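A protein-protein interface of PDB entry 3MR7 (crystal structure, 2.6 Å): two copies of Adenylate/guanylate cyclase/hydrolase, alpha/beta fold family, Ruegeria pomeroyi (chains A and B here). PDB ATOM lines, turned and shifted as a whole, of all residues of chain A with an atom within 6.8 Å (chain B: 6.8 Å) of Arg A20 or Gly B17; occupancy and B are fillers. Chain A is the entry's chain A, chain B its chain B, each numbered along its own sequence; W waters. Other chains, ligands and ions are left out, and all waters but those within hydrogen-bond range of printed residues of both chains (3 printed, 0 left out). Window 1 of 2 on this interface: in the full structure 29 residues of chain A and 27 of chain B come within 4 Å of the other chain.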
ATOM      1  N   ASP A  14      12.097 -19.805 -14.349  1.00  0.00           N
ATOM      2  CA  ASP A  14      11.005 -19.606 -13.389  1.00  0.00           C
ATOM      3  C   ASP A  14      10.611 -20.973 -12.851  1.00  0.00           C
ATOM      4  O   ASP A  14      11.044 -21.995 -13.357  1.00  0.00           O
ATOM      5  CB  ASP A  14       9.797 -18.981 -14.084  1.00  0.00           C
ATOM      6  CG  ASP A  14       8.874 -18.186 -13.138  1.00  0.00           C
ATOM      7  OD1 ASP A  14       8.944 -18.289 -11.872  1.00  0.00           O
ATOM      8  OD2 ASP A  14       8.041 -17.444 -13.716  1.00  0.00           O
ATOM      9  N   GLY A  17       4.304 -24.527 -11.753  1.00  0.00           N
ATOM     10  CA  GLY A  17       3.414 -25.286 -10.893  1.00  0.00           C
ATOM     11  C   GLY A  17       2.979 -24.576  -9.636  1.00  0.00           C
ATOM     12  O   GLY A  17       3.272 -23.403  -9.429  1.00  0.00           O
ATOM     13  N   TYR A  18       2.261 -25.309  -8.797  1.00  0.00           N
ATOM     14  CA  TYR A  18       1.842 -24.823  -7.487  1.00  0.00           C
ATOM     15  C   TYR A  18       1.026 -23.546  -7.525  1.00  0.00           C
ATOM     16  O   TYR A  18       1.325 -22.609  -6.816  1.00  0.00           O
ATOM     17  CB  TYR A  18       3.037 -24.715  -6.539  1.00  0.00           C
ATOM     18  CG  TYR A  18       3.459 -26.084  -6.067  1.00  0.00           C
ATOM     19  CD1 TYR A  18       2.744 -26.729  -5.067  1.00  0.00           C
ATOM     20  CD2 TYR A  18       4.517 -26.770  -6.662  1.00  0.00           C
ATOM     21  CE1 TYR A  18       3.080 -28.002  -4.642  1.00  0.00           C
ATOM     22  CE2 TYR A  18       4.857 -28.067  -6.245  1.00  0.00           C
ATOM     23  CZ  TYR A  18       4.129 -28.666  -5.226  1.00  0.00           C
ATOM     24  OH  TYR A  18       4.425 -29.926  -4.760  1.00  0.00           O
ATOM     25  N   SER A  19      -0.029 -23.538  -8.328  1.00  0.00           N
ATOM     26  CA  SER A  19      -0.924 -22.393  -8.406  1.00  0.00           C
ATOM     27  C   SER A  19      -1.379 -21.804  -7.051  1.00  0.00           C
ATOM     28  O   SER A  19      -1.957 -22.506  -6.199  1.00  0.00           O
ATOM     29  CB  SER A  19      -2.150 -22.740  -9.286  1.00  0.00           C
ATOM     30  OG  SER A  19      -3.127 -21.694  -9.295  1.00  0.00           O
ATOM     31  N   ARG A  20      -1.134 -20.500  -6.889  1.00  0.00           N
ATOM     32  CA  ARG A  20      -1.674 -19.662  -5.797  1.00  0.00           C
ATOM     33  C   ARG A  20      -3.210 -19.804  -5.585  1.00  0.00           C
ATOM     34  O   ARG A  20      -3.772 -19.288  -4.620  1.00  0.00           O
ATOM     35  CB  ARG A  20      -1.361 -18.184  -6.104  1.00  0.00           C
ATOM     36  CG  ARG A  20      -0.125 -17.548  -5.435  1.00  0.00           C
ATOM     37  CD  ARG A  20       1.178 -18.237  -5.725  1.00  0.00           C
ATOM     38  NE  ARG A  20       1.957 -17.577  -6.760  1.00  0.00           N
ATOM     39  CZ  ARG A  20       3.034 -16.840  -6.530  1.00  0.00           C
ATOM     40  NH1 ARG A  20       3.466 -16.642  -5.293  1.00  0.00           N
ATOM     41  NH2 ARG A  20       3.680 -16.298  -7.548  1.00  0.00           N
ATOM     42  N   LEU A  21      -3.891 -20.477  -6.505  1.00  0.00           N
ATOM     43  CA  LEU A  21      -5.325 -20.581  -6.436  1.00  0.00           C
ATOM     44  C   LEU A  21      -5.677 -21.788  -5.634  1.00  0.00           C
ATOM     45  O   LEU A  21      -6.833 -21.970  -5.308  1.00  0.00           O
ATOM     46  CB  LEU A  21      -5.921 -20.714  -7.828  1.00  0.00           C
ATOM     47  CG  LEU A  21      -6.276 -19.424  -8.572  1.00  0.00           C
ATOM     48  CD1 LEU A  21      -5.057 -18.551  -8.747  1.00  0.00           C
ATOM     49  CD2 LEU A  21      -6.872 -19.759  -9.920  1.00  0.00           C
ATOM     50  N   MET A  22      -4.682 -22.630  -5.342  1.00  0.00           N
ATOM     51  CA  MET A  22      -4.829 -23.684  -4.336  1.00  0.00           C
ATOM     52  C   MET A  22      -5.099 -23.018  -2.980  1.00  0.00           C
ATOM     53  O   MET A  22      -5.442 -23.686  -1.991  1.00  0.00           O
ATOM     54  CB  MET A  22      -3.574 -24.563  -4.261  1.00  0.00           C
ATOM     55  CG  MET A  22      -3.566 -25.728  -5.236  1.00  0.00           C
ATOM     56  SD  MET A  22      -5.206 -26.477  -5.287  1.00  0.00           S
ATOM     57  CE  MET A  22      -4.940 -27.987  -4.365  1.00  0.00           C
ATOM     58  N   GLU A  23      -4.951 -21.689  -2.948  1.00  0.00           N
ATOM     59  CA  GLU A  23      -5.221 -20.904  -1.743  1.00  0.00           C
ATOM     60  C   GLU A  23      -4.468 -21.520  -0.573  1.00  0.00           C
ATOM     61  O   GLU A  23      -5.012 -21.648   0.525  1.00  0.00           O
ATOM     62  CB  GLU A  23      -6.733 -20.839  -1.426  1.00  0.00           C
ATOM     63  CG  GLU A  23      -7.543 -19.854  -2.283  1.00  0.00           C
ATOM     64  CD  GLU A  23      -9.041 -19.869  -1.982  1.00  0.00           C
ATOM     65  OE1 GLU A  23      -9.435 -20.265  -0.862  1.00  0.00           O
ATOM     66  OE2 GLU A  23      -9.830 -19.473  -2.870  1.00  0.00           O
ATOM     67  N   ARG A  24      -3.219 -21.915  -0.802  1.00  0.00           N
ATOM     68  CA  ARG A  24      -2.453 -22.505   0.277  1.00  0.00           C
ATOM     69  C   ARG A  24      -0.944 -22.169   0.313  1.00  0.00           C
ATOM     70  O   ARG A  24      -0.262 -22.110  -0.711  1.00  0.00           O
ATOM     71  CB  ARG A  24      -2.777 -23.994   0.373  1.00  0.00           C
ATOM     72  CG  ARG A  24      -1.648 -24.915   0.143  1.00  0.00           C
ATOM     73  CD  ARG A  24      -2.020 -26.278   0.703  1.00  0.00           C
ATOM     74  NE  ARG A  24      -3.333 -26.723   0.243  1.00  0.00           N
ATOM     75  CZ  ARG A  24      -3.525 -27.556  -0.776  1.00  0.00           C
ATOM     76  NH1 ARG A  24      -2.484 -28.039  -1.444  1.00  0.00           N
ATOM     77  NH2 ARG A  24      -4.757 -27.909  -1.126  1.00  0.00           N
ATOM     78  N   LEU A  30       8.098 -24.278  -0.948  1.00  0.00           N
ATOM     79  CA  LEU A  30       8.842 -23.030  -1.125  1.00  0.00           C
ATOM     80  C   LEU A  30      10.238 -23.084  -0.491  1.00  0.00           C
ATOM     81  O   LEU A  30      11.160 -22.421  -0.967  1.00  0.00           O
ATOM     82  CB  LEU A  30       8.055 -21.845  -0.572  1.00  0.00           C
ATOM     83  CG  LEU A  30       6.630 -21.649  -1.098  1.00  0.00           C
ATOM     84  CD1 LEU A  30       5.969 -20.548  -0.315  1.00  0.00           C
ATOM     85  CD2 LEU A  30       6.620 -21.309  -2.583  1.00  0.00           C
ATOM     86  N   GLY A  57       9.625 -10.406 -10.296  1.00  0.00           N
ATOM     87  CA  GLY A  57       8.368 -11.116 -10.319  1.00  0.00           C
ATOM     88  C   GLY A  57       8.282 -12.037 -11.518  1.00  0.00           C
ATOM     89  O   GLY A  57       7.488 -12.978 -11.534  1.00  0.00           O
ATOM     90  N   ASP A  58       9.113 -11.755 -12.519  1.00  0.00           N
ATOM     91  CA  ASP A  58       9.103 -12.469 -13.791  1.00  0.00           C
ATOM     92  C   ASP A  58       9.982 -13.692 -13.700  1.00  0.00           C
ATOM     93  O   ASP A  58       9.991 -14.529 -14.599  1.00  0.00           O
ATOM     94  CB  ASP A  58       9.633 -11.569 -14.925  1.00  0.00           C
ATOM     95  CG  ASP A  58       8.643 -10.450 -15.335  1.00  0.00           C
ATOM     96  OD1 ASP A  58       7.417 -10.632 -15.155  1.00  0.00           O
ATOM     97  OD2 ASP A  58       9.099  -9.395 -15.860  1.00  0.00           O
ATOM     98  N   ASP B  14      -5.068 -19.242 -14.418  1.00  0.00           N
ATOM     99  CA  ASP B  14      -4.060 -19.242 -13.363  1.00  0.00           C
ATOM    100  C   ASP B  14      -3.625 -17.817 -13.089  1.00  0.00           C
ATOM    101  O   ASP B  14      -4.030 -16.900 -13.806  1.00  0.00           O
ATOM    102  CB  ASP B  14      -2.862 -20.152 -13.700  1.00  0.00           C
ATOM    103  CG  ASP B  14      -2.067 -20.556 -12.455  1.00  0.00           C
ATOM    104  OD1 ASP B  14      -2.464 -20.137 -11.348  1.00  0.00           O
ATOM    105  OD2 ASP B  14      -1.057 -21.288 -12.571  1.00  0.00           O
ATOM    106  N   MET B  15      -2.831 -17.627 -12.033  1.00  0.00           N
ATOM    107  CA  MET B  15      -2.337 -16.290 -11.674  1.00  0.00           C
ATOM    108  C   MET B  15      -0.937 -16.036 -12.231  1.00  0.00           C
ATOM    109  O   MET B  15      -0.060 -16.872 -12.109  1.00  0.00           O
ATOM    110  CB  MET B  15      -2.325 -16.102 -10.165  1.00  0.00           C
ATOM    111  CG  MET B  15      -2.387 -14.644  -9.730  1.00  0.00           C
ATOM    112  SD  MET B  15      -1.742 -14.314  -7.883  1.00  0.00           S
ATOM    113  CE  MET B  15      -0.038 -15.254  -7.993  1.00  0.00           C
ATOM    114  N   ALA B  16      -0.734 -14.883 -12.852  1.00  0.00           N
ATOM    115  CA  ALA B  16       0.584 -14.542 -13.390  1.00  0.00           C
ATOM    116  C   ALA B  16       1.470 -13.935 -12.324  1.00  0.00           C
ATOM    117  O   ALA B  16       0.984 -13.498 -11.290  1.00  0.00           O
ATOM    118  CB  ALA B  16       0.436 -13.559 -14.503  1.00  0.00           C
ATOM    119  N   GLY B  17       2.769 -13.903 -12.582  1.00  0.00           N
ATOM    120  CA  GLY B  17       3.658 -13.038 -11.835  1.00  0.00           C
ATOM    121  C   GLY B  17       4.057 -13.578 -10.494  1.00  0.00           C
ATOM    122  O   GLY B  17       3.861 -14.748 -10.241  1.00  0.00           O
ATOM    123  N   TYR B  18       4.642 -12.723  -9.661  1.00  0.00           N
ATOM    124  CA  TYR B  18       5.140 -13.086  -8.329  1.00  0.00           C
ATOM    125  C   TYR B  18       5.979 -14.352  -8.307  1.00  0.00           C
ATOM    126  O   TYR B  18       5.852 -15.181  -7.401  1.00  0.00           O
ATOM    127  CB  TYR B  18       4.002 -13.166  -7.294  1.00  0.00           C
ATOM    128  CG  TYR B  18       3.327 -11.850  -7.089  1.00  0.00           C
ATOM    129  CD1 TYR B  18       3.612 -11.065  -5.972  1.00  0.00           C
ATOM    130  CD2 TYR B  18       2.436 -11.363  -8.027  1.00  0.00           C
ATOM    131  CE1 TYR B  18       3.005  -9.827  -5.792  1.00  0.00           C
ATOM    132  CE2 TYR B  18       1.849 -10.115  -7.866  1.00  0.00           C
ATOM    133  CZ  TYR B  18       2.125  -9.359  -6.751  1.00  0.00           C
ATOM    134  OH  TYR B  18       1.505  -8.138  -6.599  1.00  0.00           O
ATOM    135  N   SER B  19       6.859 -14.481  -9.286  1.00  0.00           N
ATOM    136  CA  SER B  19       7.780 -15.603  -9.302  1.00  0.00           C
ATOM    137  C   SER B  19       8.270 -15.968  -7.896  1.00  0.00           C
ATOM    138  O   SER B  19       8.555 -15.096  -7.078  1.00  0.00           O
ATOM    139  CB  SER B  19       8.968 -15.308 -10.219  1.00  0.00           C
ATOM    140  OG  SER B  19       9.989 -16.267 -10.028  1.00  0.00           O
ATOM    141  N   ARG B  20       8.378 -17.257  -7.619  1.00  0.00           N
ATOM    142  CA  ARG B  20       8.782 -17.670  -6.299  1.00  0.00           C
ATOM    143  C   ARG B  20      10.255 -17.667  -6.232  1.00  0.00           C
ATOM    144  O   ARG B  20      10.820 -17.985  -5.210  1.00  0.00           O
ATOM    145  CB  ARG B  20       8.286 -19.051  -6.002  1.00  0.00           C
ATOM    146  CG  ARG B  20       6.795 -19.145  -6.025  1.00  0.00           C
ATOM    147  CD  ARG B  20       6.439 -20.578  -5.995  1.00  0.00           C
ATOM    148  NE  ARG B  20       5.308 -20.806  -6.864  1.00  0.00           N
ATOM    149  CZ  ARG B  20       4.056 -20.684  -6.464  1.00  0.00           C
ATOM    150  NH1 ARG B  20       3.789 -20.356  -5.193  1.00  0.00           N
ATOM    151  NH2 ARG B  20       3.086 -20.902  -7.342  1.00  0.00           N
ATOM    152  N   MET B  22      11.715 -15.158  -6.136  1.00  0.00           N
ATOM    153  CA  MET B  22      11.998 -13.968  -5.346  1.00  0.00           C
ATOM    154  C   MET B  22      12.075 -14.276  -3.851  1.00  0.00           C
ATOM    155  O   MET B  22      12.864 -13.684  -3.126  1.00  0.00           O
ATOM    156  CB  MET B  22      10.985 -12.882  -5.627  1.00  0.00           C
ATOM    157  CG  MET B  22      11.604 -11.634  -6.187  1.00  0.00           C
ATOM    158  SD  MET B  22      10.118 -10.619  -6.904  1.00  0.00           S
ATOM    159  CE  MET B  22       8.637 -11.825  -6.424  1.00  0.00           C
ATOM    160  N   ARG B  24       9.881 -13.863  -1.651  1.00  0.00           N
ATOM    161  CA  ARG B  24       9.003 -12.992  -0.886  1.00  0.00           C
ATOM    162  C   ARG B  24       7.933 -13.778  -0.107  1.00  0.00           C
ATOM    163  O   ARG B  24       7.669 -14.961  -0.368  1.00  0.00           O
ATOM    164  CB  ARG B  24       8.350 -11.961  -1.813  1.00  0.00           C
ATOM    165  CG  ARG B  24       7.884 -10.663  -1.146  1.00  0.00           C
ATOM    166  CD  ARG B  24       7.793  -9.574  -2.201  1.00  0.00           C
ATOM    167  NE  ARG B  24       9.070  -9.481  -2.894  1.00  0.00           N
ATOM    168  CZ  ARG B  24       9.831  -8.393  -2.933  1.00  0.00           C
ATOM    169  NH1 ARG B  24       9.424  -7.275  -2.345  1.00  0.00           N
ATOM    170  NH2 ARG B  24      10.995  -8.415  -3.576  1.00  0.00           N
ATOM    171  N   ASN B  25       7.328 -13.098   0.861  1.00  0.00           N
ATOM    172  CA  ASN B  25       6.288 -13.670   1.702  1.00  0.00           C
ATOM    173  C   ASN B  25       5.036 -13.973   0.897  1.00  0.00           C
ATOM    174  O   ASN B  25       4.377 -13.068   0.363  1.00  0.00           O
ATOM    175  CB  ASN B  25       5.951 -12.709   2.834  1.00  0.00           C
ATOM    176  CG  ASN B  25       5.100 -13.347   3.894  1.00  0.00           C
ATOM    177  OD1 ASN B  25       4.750 -14.523   3.803  1.00  0.00           O
ATOM    178  ND2 ASN B  25       4.766 -12.577   4.920  1.00  0.00           N
ATOM    179  N   GLU B  26       4.706 -15.253   0.816  1.00  0.00           N
ATOM    180  CA  GLU B  26       3.579 -15.660  -0.010  1.00  0.00           C
ATOM    181  C   GLU B  26       2.288 -15.132   0.582  1.00  0.00           C
ATOM    182  O   GLU B  26       1.418 -14.638  -0.143  1.00  0.00           O
ATOM    183  CB  GLU B  26       3.514 -17.174  -0.143  1.00  0.00           C
ATOM    184  CG  GLU B  26       4.584 -17.746  -1.031  1.00  0.00           C
ATOM    185  CD  GLU B  26       4.177 -17.772  -2.469  1.00  0.00           C
ATOM    186  OE1 GLU B  26       3.526 -18.761  -2.880  1.00  0.00           O
ATOM    187  OE2 GLU B  26       4.507 -16.802  -3.184  1.00  0.00           O
ATOM    188  N   VAL B  29       0.168 -11.972  -1.004  1.00  0.00           N
ATOM    189  CA  VAL B  29      -0.408 -12.218  -2.323  1.00  0.00           C
ATOM    190  C   VAL B  29      -1.517 -13.303  -2.326  1.00  0.00           C
ATOM    191  O   VAL B  29      -2.537 -13.163  -3.009  1.00  0.00           O
ATOM    192  CB  VAL B  29       0.701 -12.525  -3.399  1.00  0.00           C
ATOM    193  CG1 VAL B  29       1.526 -13.752  -3.029  1.00  0.00           C
ATOM    194  CG2 VAL B  29       0.092 -12.686  -4.783  1.00  0.00           C
ATOM    195  N   LEU B  30      -1.333 -14.371  -1.557  1.00  0.00           N
ATOM    196  CA  LEU B  30      -2.372 -15.383  -1.442  1.00  0.00           C
ATOM    197  C   LEU B  30      -3.701 -14.747  -1.078  1.00  0.00           C
ATOM    198  O   LEU B  30      -4.722 -15.059  -1.677  1.00  0.00           O
ATOM    199  CB  LEU B  30      -1.999 -16.443  -0.409  1.00  0.00           C
ATOM    200  CG  LEU B  30      -0.945 -17.465  -0.833  1.00  0.00           C
ATOM    201  CD1 LEU B  30      -0.251 -18.115   0.379  1.00  0.00           C
ATOM    202  CD2 LEU B  30      -1.584 -18.513  -1.767  1.00  0.00           C
ATOM    203  N   GLN B  33      -5.480 -12.661  -3.934  1.00  0.00           N
ATOM    204  CA  GLN B  33      -6.041 -13.500  -4.965  1.00  0.00           C
ATOM    205  C   GLN B  33      -7.259 -14.191  -4.364  1.00  0.00           C
ATOM    206  O   GLN B  33      -8.290 -14.324  -5.019  1.00  0.00           O
ATOM    207  CB  GLN B  33      -4.996 -14.479  -5.531  1.00  0.00           C
ATOM    208  CG  GLN B  33      -5.247 -15.967  -5.277  1.00  0.00           C
ATOM    209  CD  GLN B  33      -6.446 -16.516  -6.035  1.00  0.00           C
ATOM    210  OE1 GLN B  33      -6.713 -16.135  -7.170  1.00  0.00           O
ATOM    211  NE2 GLN B  33      -7.175 -17.417  -5.402  1.00  0.00           N
ATOM    212  N   LYS B  34      -7.149 -14.590  -3.100  1.00  0.00           N
ATOM    213  CA  LYS B  34      -8.255 -15.256  -2.402  1.00  0.00           C
ATOM    214  C   LYS B  34      -9.507 -14.374  -2.405  1.00  0.00           C
ATOM    215  O   LYS B  34     -10.631 -14.864  -2.407  1.00  0.00           O
ATOM    216  CB  LYS B  34      -7.840 -15.619  -0.976  1.00  0.00           C
ATOM    217  CG  LYS B  34      -8.862 -16.375  -0.190  1.00  0.00           C
ATOM    218  CD  LYS B  34      -8.289 -16.774   1.155  1.00  0.00           C
ATOM    219  CE  LYS B  34      -9.317 -17.565   1.978  1.00  0.00           C
ATOM    220  NZ  LYS B  34      -8.774 -18.156   3.241  1.00  0.00           N
ATOM    221  N   THR B  55      -9.868 -27.089  -8.677  1.00  0.00           N
ATOM    222  CA  THR B  55      -8.637 -26.304  -8.684  1.00  0.00           C
ATOM    223  C   THR B  55      -7.458 -27.168  -8.285  1.00  0.00           C
ATOM    224  O   THR B  55      -7.592 -28.044  -7.455  1.00  0.00           O
ATOM    225  CB  THR B  55      -8.710 -25.118  -7.730  1.00  0.00           C
ATOM    226  OG1 THR B  55      -9.849 -24.318  -8.070  1.00  0.00           O
ATOM    227  CG2 THR B  55      -7.438 -24.276  -7.845  1.00  0.00           C
ATOM    228  N   THR B  56      -6.304 -26.944  -8.889  1.00  0.00           N
ATOM    229  CA  THR B  56      -5.130 -27.735  -8.549  1.00  0.00           C
ATOM    230  C   THR B  56      -3.891 -26.884  -8.703  1.00  0.00           C
ATOM    231  O   THR B  56      -3.989 -25.667  -8.874  1.00  0.00           O
ATOM    232  CB  THR B  56      -4.981 -28.960  -9.460  1.00  0.00           C
ATOM    233  OG1 THR B  56      -4.707 -28.536 -10.808  1.00  0.00           O
ATOM    234  CG2 THR B  56      -6.235 -29.829  -9.427  1.00  0.00           C
ATOM    235  N   GLY B  57      -2.734 -27.540  -8.656  1.00  0.00           N
ATOM    236  CA  GLY B  57      -1.455 -26.889  -8.821  1.00  0.00           C
ATOM    237  C   GLY B  57      -1.346 -26.243 -10.185  1.00  0.00           C
ATOM    238  O   GLY B  57      -0.518 -25.350 -10.408  1.00  0.00           O
ATOM    239  N   ARG B  93       0.682  -5.524  -9.042  1.00  0.00           N
ATOM    240  CA  ARG B  93      -0.672  -5.899  -9.460  1.00  0.00           C
ATOM    241  C   ARG B  93      -0.890  -7.399  -9.474  1.00  0.00           C
ATOM    242  O   ARG B  93       0.057  -8.176  -9.531  1.00  0.00           O
ATOM    243  CB  ARG B  93      -0.979  -5.366 -10.847  1.00  0.00           C
ATOM    244  CG  ARG B  93      -1.798  -4.123 -10.830  1.00  0.00           C
ATOM    245  CD  ARG B  93      -1.739  -3.438 -12.163  1.00  0.00           C
ATOM    246  NE  ARG B  93      -1.897  -2.001 -12.012  1.00  0.00           N
ATOM    247  CZ  ARG B  93      -1.776  -1.141 -13.011  1.00  0.00           C
ATOM    248  NH1 ARG B  93      -1.505  -1.583 -14.227  1.00  0.00           N
ATOM    249  NH2 ARG B  93      -1.942   0.155 -12.800  1.00  0.00           N
ATOM    250  N   GLN B  95      -2.742 -10.430 -11.628  1.00  0.00           N
ATOM    251  CA  GLN B  95      -3.333 -10.716 -12.927  1.00  0.00           C
ATOM    252  C   GLN B  95      -3.465 -12.205 -13.194  1.00  0.00           C
ATOM    253  O   GLN B  95      -2.631 -13.021 -12.750  1.00  0.00           O
ATOM    254  CB  GLN B  95      -2.489 -10.127 -14.044  1.00  0.00           C
ATOM    255  CG  GLN B  95      -2.262  -8.642 -14.025  1.00  0.00           C
ATOM    256  CD  GLN B  95      -1.331  -8.256 -15.158  1.00  0.00           C
ATOM    257  OE1 GLN B  95      -0.175  -8.664 -15.177  1.00  0.00           O
ATOM    258  NE2 GLN B  95      -1.845  -7.531 -16.135  1.00  0.00           N
ATOM    259  N   ARG B  97      -4.087 -15.325 -16.216  1.00  0.00           N
ATOM    260  CA  ARG B  97      -4.049 -15.745 -17.606  1.00  0.00           C
ATOM    261  C   ARG B  97      -5.252 -16.650 -17.742  1.00  0.00           C
ATOM    262  O   ARG B  97      -5.565 -17.401 -16.810  1.00  0.00           O
ATOM    263  CB  ARG B  97      -2.794 -16.546 -17.919  1.00  0.00           C
ATOM    264  CG  ARG B  97      -1.513 -15.831 -17.672  1.00  0.00           C
ATOM    265  CD  ARG B  97      -0.342 -16.617 -18.227  1.00  0.00           C
ATOM    266  NE  ARG B  97      -0.153 -17.900 -17.561  1.00  0.00           N
ATOM    267  CZ  ARG B  97       0.496 -18.041 -16.413  1.00  0.00           C
ATOM    268  NH1 ARG B  97       1.020 -16.982 -15.818  1.00  0.00           N
ATOM    269  NH2 ARG B  97       0.624 -19.230 -15.862  1.00  0.00           N
ATOM    270  N   PRO B 129      -0.317 -12.146 -19.409  1.00  0.00           N
ATOM    271  CA  PRO B 129      -0.957 -11.814 -18.135  1.00  0.00           C
ATOM    272  C   PRO B 129      -2.106 -10.822 -18.349  1.00  0.00           C
ATOM    273  O   PRO B 129      -1.921  -9.768 -18.948  1.00  0.00           O
ATOM    274  CB  PRO B 129       0.182 -11.165 -17.350  1.00  0.00           C
ATOM    275  CG  PRO B 129       1.372 -11.818 -17.870  1.00  0.00           C
ATOM    276  CD  PRO B 129       1.137 -11.954 -19.349  1.00  0.00           C
HETATM  277  O   HOH W   1       7.294 -18.773  -9.577  1.00  0.00           O
HETATM  278  O   HOH W   2       5.344 -20.985  -9.473  1.00  0.00           O
HETATM  279  O   HOH W   3      -8.697 -19.706  -5.371  1.00  0.00           O
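Water W2 lies within hydrogen-bond range of the guanidinium group of Arg B20 (2.6 Å) and the backbone carbonyl oxygen of Gly A17 (3.2 Å). Water W1 bridges the backbone NH of Arg B20 and the side-chain carboxylate of Asp A14. Water W3 lies within hydrogen-bond range of the side-chain amide nitrogen of Gln B33, the side-chain carboxylate of Glu A23 and the backbone carbonyl oxygen of Leu A21.
Asp A14 touches Ser B19, and with the chains exchanged Ser A19 touches Asp B14. Gly A17 touches Gly B57, and with the chains exchanged Gly A57 touches Gly B17. Arg A20 touches Leu B30, and with the chains exchanged Leu A30 touches Arg B20. Met A22 touches Gly B57, and with the chains exchanged Gly A57 touches Met B22. 9 positions are printed for both chains. Of the 31 pairs that touch across the chains among the printed residues, 17 have their exchanged pair printed and touching as well.
Ser A19 touches Thr B56 (CB to O, 3.5 Å). CE of Met B15 touches NE of Arg A20 (3.3 Å). Leu B30 touches Arg A20 (CD2 to O, 3.7 Å). CG of Gln B33 touches O of Arg A20, at 3.7 Å. Leu A21 touches Gln B33 (CD1 to OE1, 3.3 Å). Gly B57 touches Met A22. Glu A23 touches Gln B33. Leu B30 touches Arg A24 (CD2 to N, 3.9 Å). CD of Arg B20 touches CD2 of Leu A30 (3.5 Å). Gly A57 touches Gly B17.
Printed residues of chain B within 4 Å of Tyr A18: Arg B20 (2.5 Å) and Gly B57 (3.2 Å). Of the printed residues of chain B, Leu A21 touches Met B15 (3.9 Å), Gln B33 (3.3 Å) and Thr B55 (3.5 Å). Of chain A, only Arg A20 and Gly A57 come within 4 Å of Gly B17. Printed residues of chain A within 4 Å of Glu B26: Arg A20 and Leu A30. Of the printed residues of chain A, Leu B30 touches Arg A20 and Arg A24. Of the printed residues of chain A, Lys B34 touches Glu A23. Arg B93 touches none of the printed residues of chain A. The nearest residue of chain B that does not touch Arg A20 is Ser B19 (4.1 Å). The nearest printed residue of chain B that does not touch Glu A23 is Leu B30 (4.3 Å).
The side-chain sulfur of Met A22 lies close to the backbone NH of Thr B56 (3.8 Å). NH2 of Arg A20 lies within hydrogen-bond range of O of Gly B17 (3.1 Å). The backbone carbonyl oxygen (O) of Tyr A18 is in hydrogen-bond range of the guanidinium group (NH2) of Arg B20, 2.5 Å away. The backbone NH of Tyr A18 is in hydrogen-bond range of the backbone carbonyl oxygen of Gly B57. OE1 of Glu B26 is in salt-bridge range of NH1 of Arg A20 (3.2 Å). The backbone carbonyl oxygen (O) of Gly A57 is in hydrogen-bond range of the backbone NH (N) of Tyr B18, at 3.4 Å. The guanidinium group (NH2) of Arg A20 sits at hydrogen-bond distance from the backbone carbonyl oxygen (O) of Tyr B18 (2.4 Å). O of Gly A57 sits at hydrogen-bond distance from N of Ser B19. The side-chain sulfur (SD) of Met A22 sits close to the backbone carbonyl oxygen (O) of Thr B55. N of Ser A19 lies within hydrogen-bond range of O of Gly B57 (2.8 Å). OG of Ser A19 is in hydrogen-bond range of OD1 of Asp B14, at 2.7 Å. The side-chain sulfur of Met B22 sits at hydrogen-bond distance from the backbone NH of Gly A57 (3.4 Å). The side-chain carboxylate (OD1) of Asp A14 is in hydrogen-bond range of the side-chain hydroxyl (OG) of Ser B19. The backbone carbonyl oxygen (O) of Gly A17 lies within hydrogen-bond range of the guanidinium group (NH2) of Arg B20 (3.3 Å).
Of the 22 printed residues of chain B, 14 touch a printed residue of chain A. Among the printed residues, 31 pairs touch across the chains. Among the printed residues, Asp or Glu carboxylates within 4 Å of a Lys or Arg side-chain nitrogen of the other chain: Arg A20 with Glu B26.
The side-chain hydroxyl (OH) of Tyr B18 sits close to the backbone carbonyl oxygen (O) of Arg B93. The backbone NH of Leu A21 sits close to the side-chain hydroxyl of Ser A19 (3.1 Å). The guanidinium group (NH1) of Arg B20 lies within salt-bridge range of the side-chain carboxylate (OE1) of Glu B26, 2.8 Å away. The backbone carbonyl oxygen of Asp B14 sits at hydrogen-bond distance from the backbone NH of Arg B97, at 2.9 Å.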
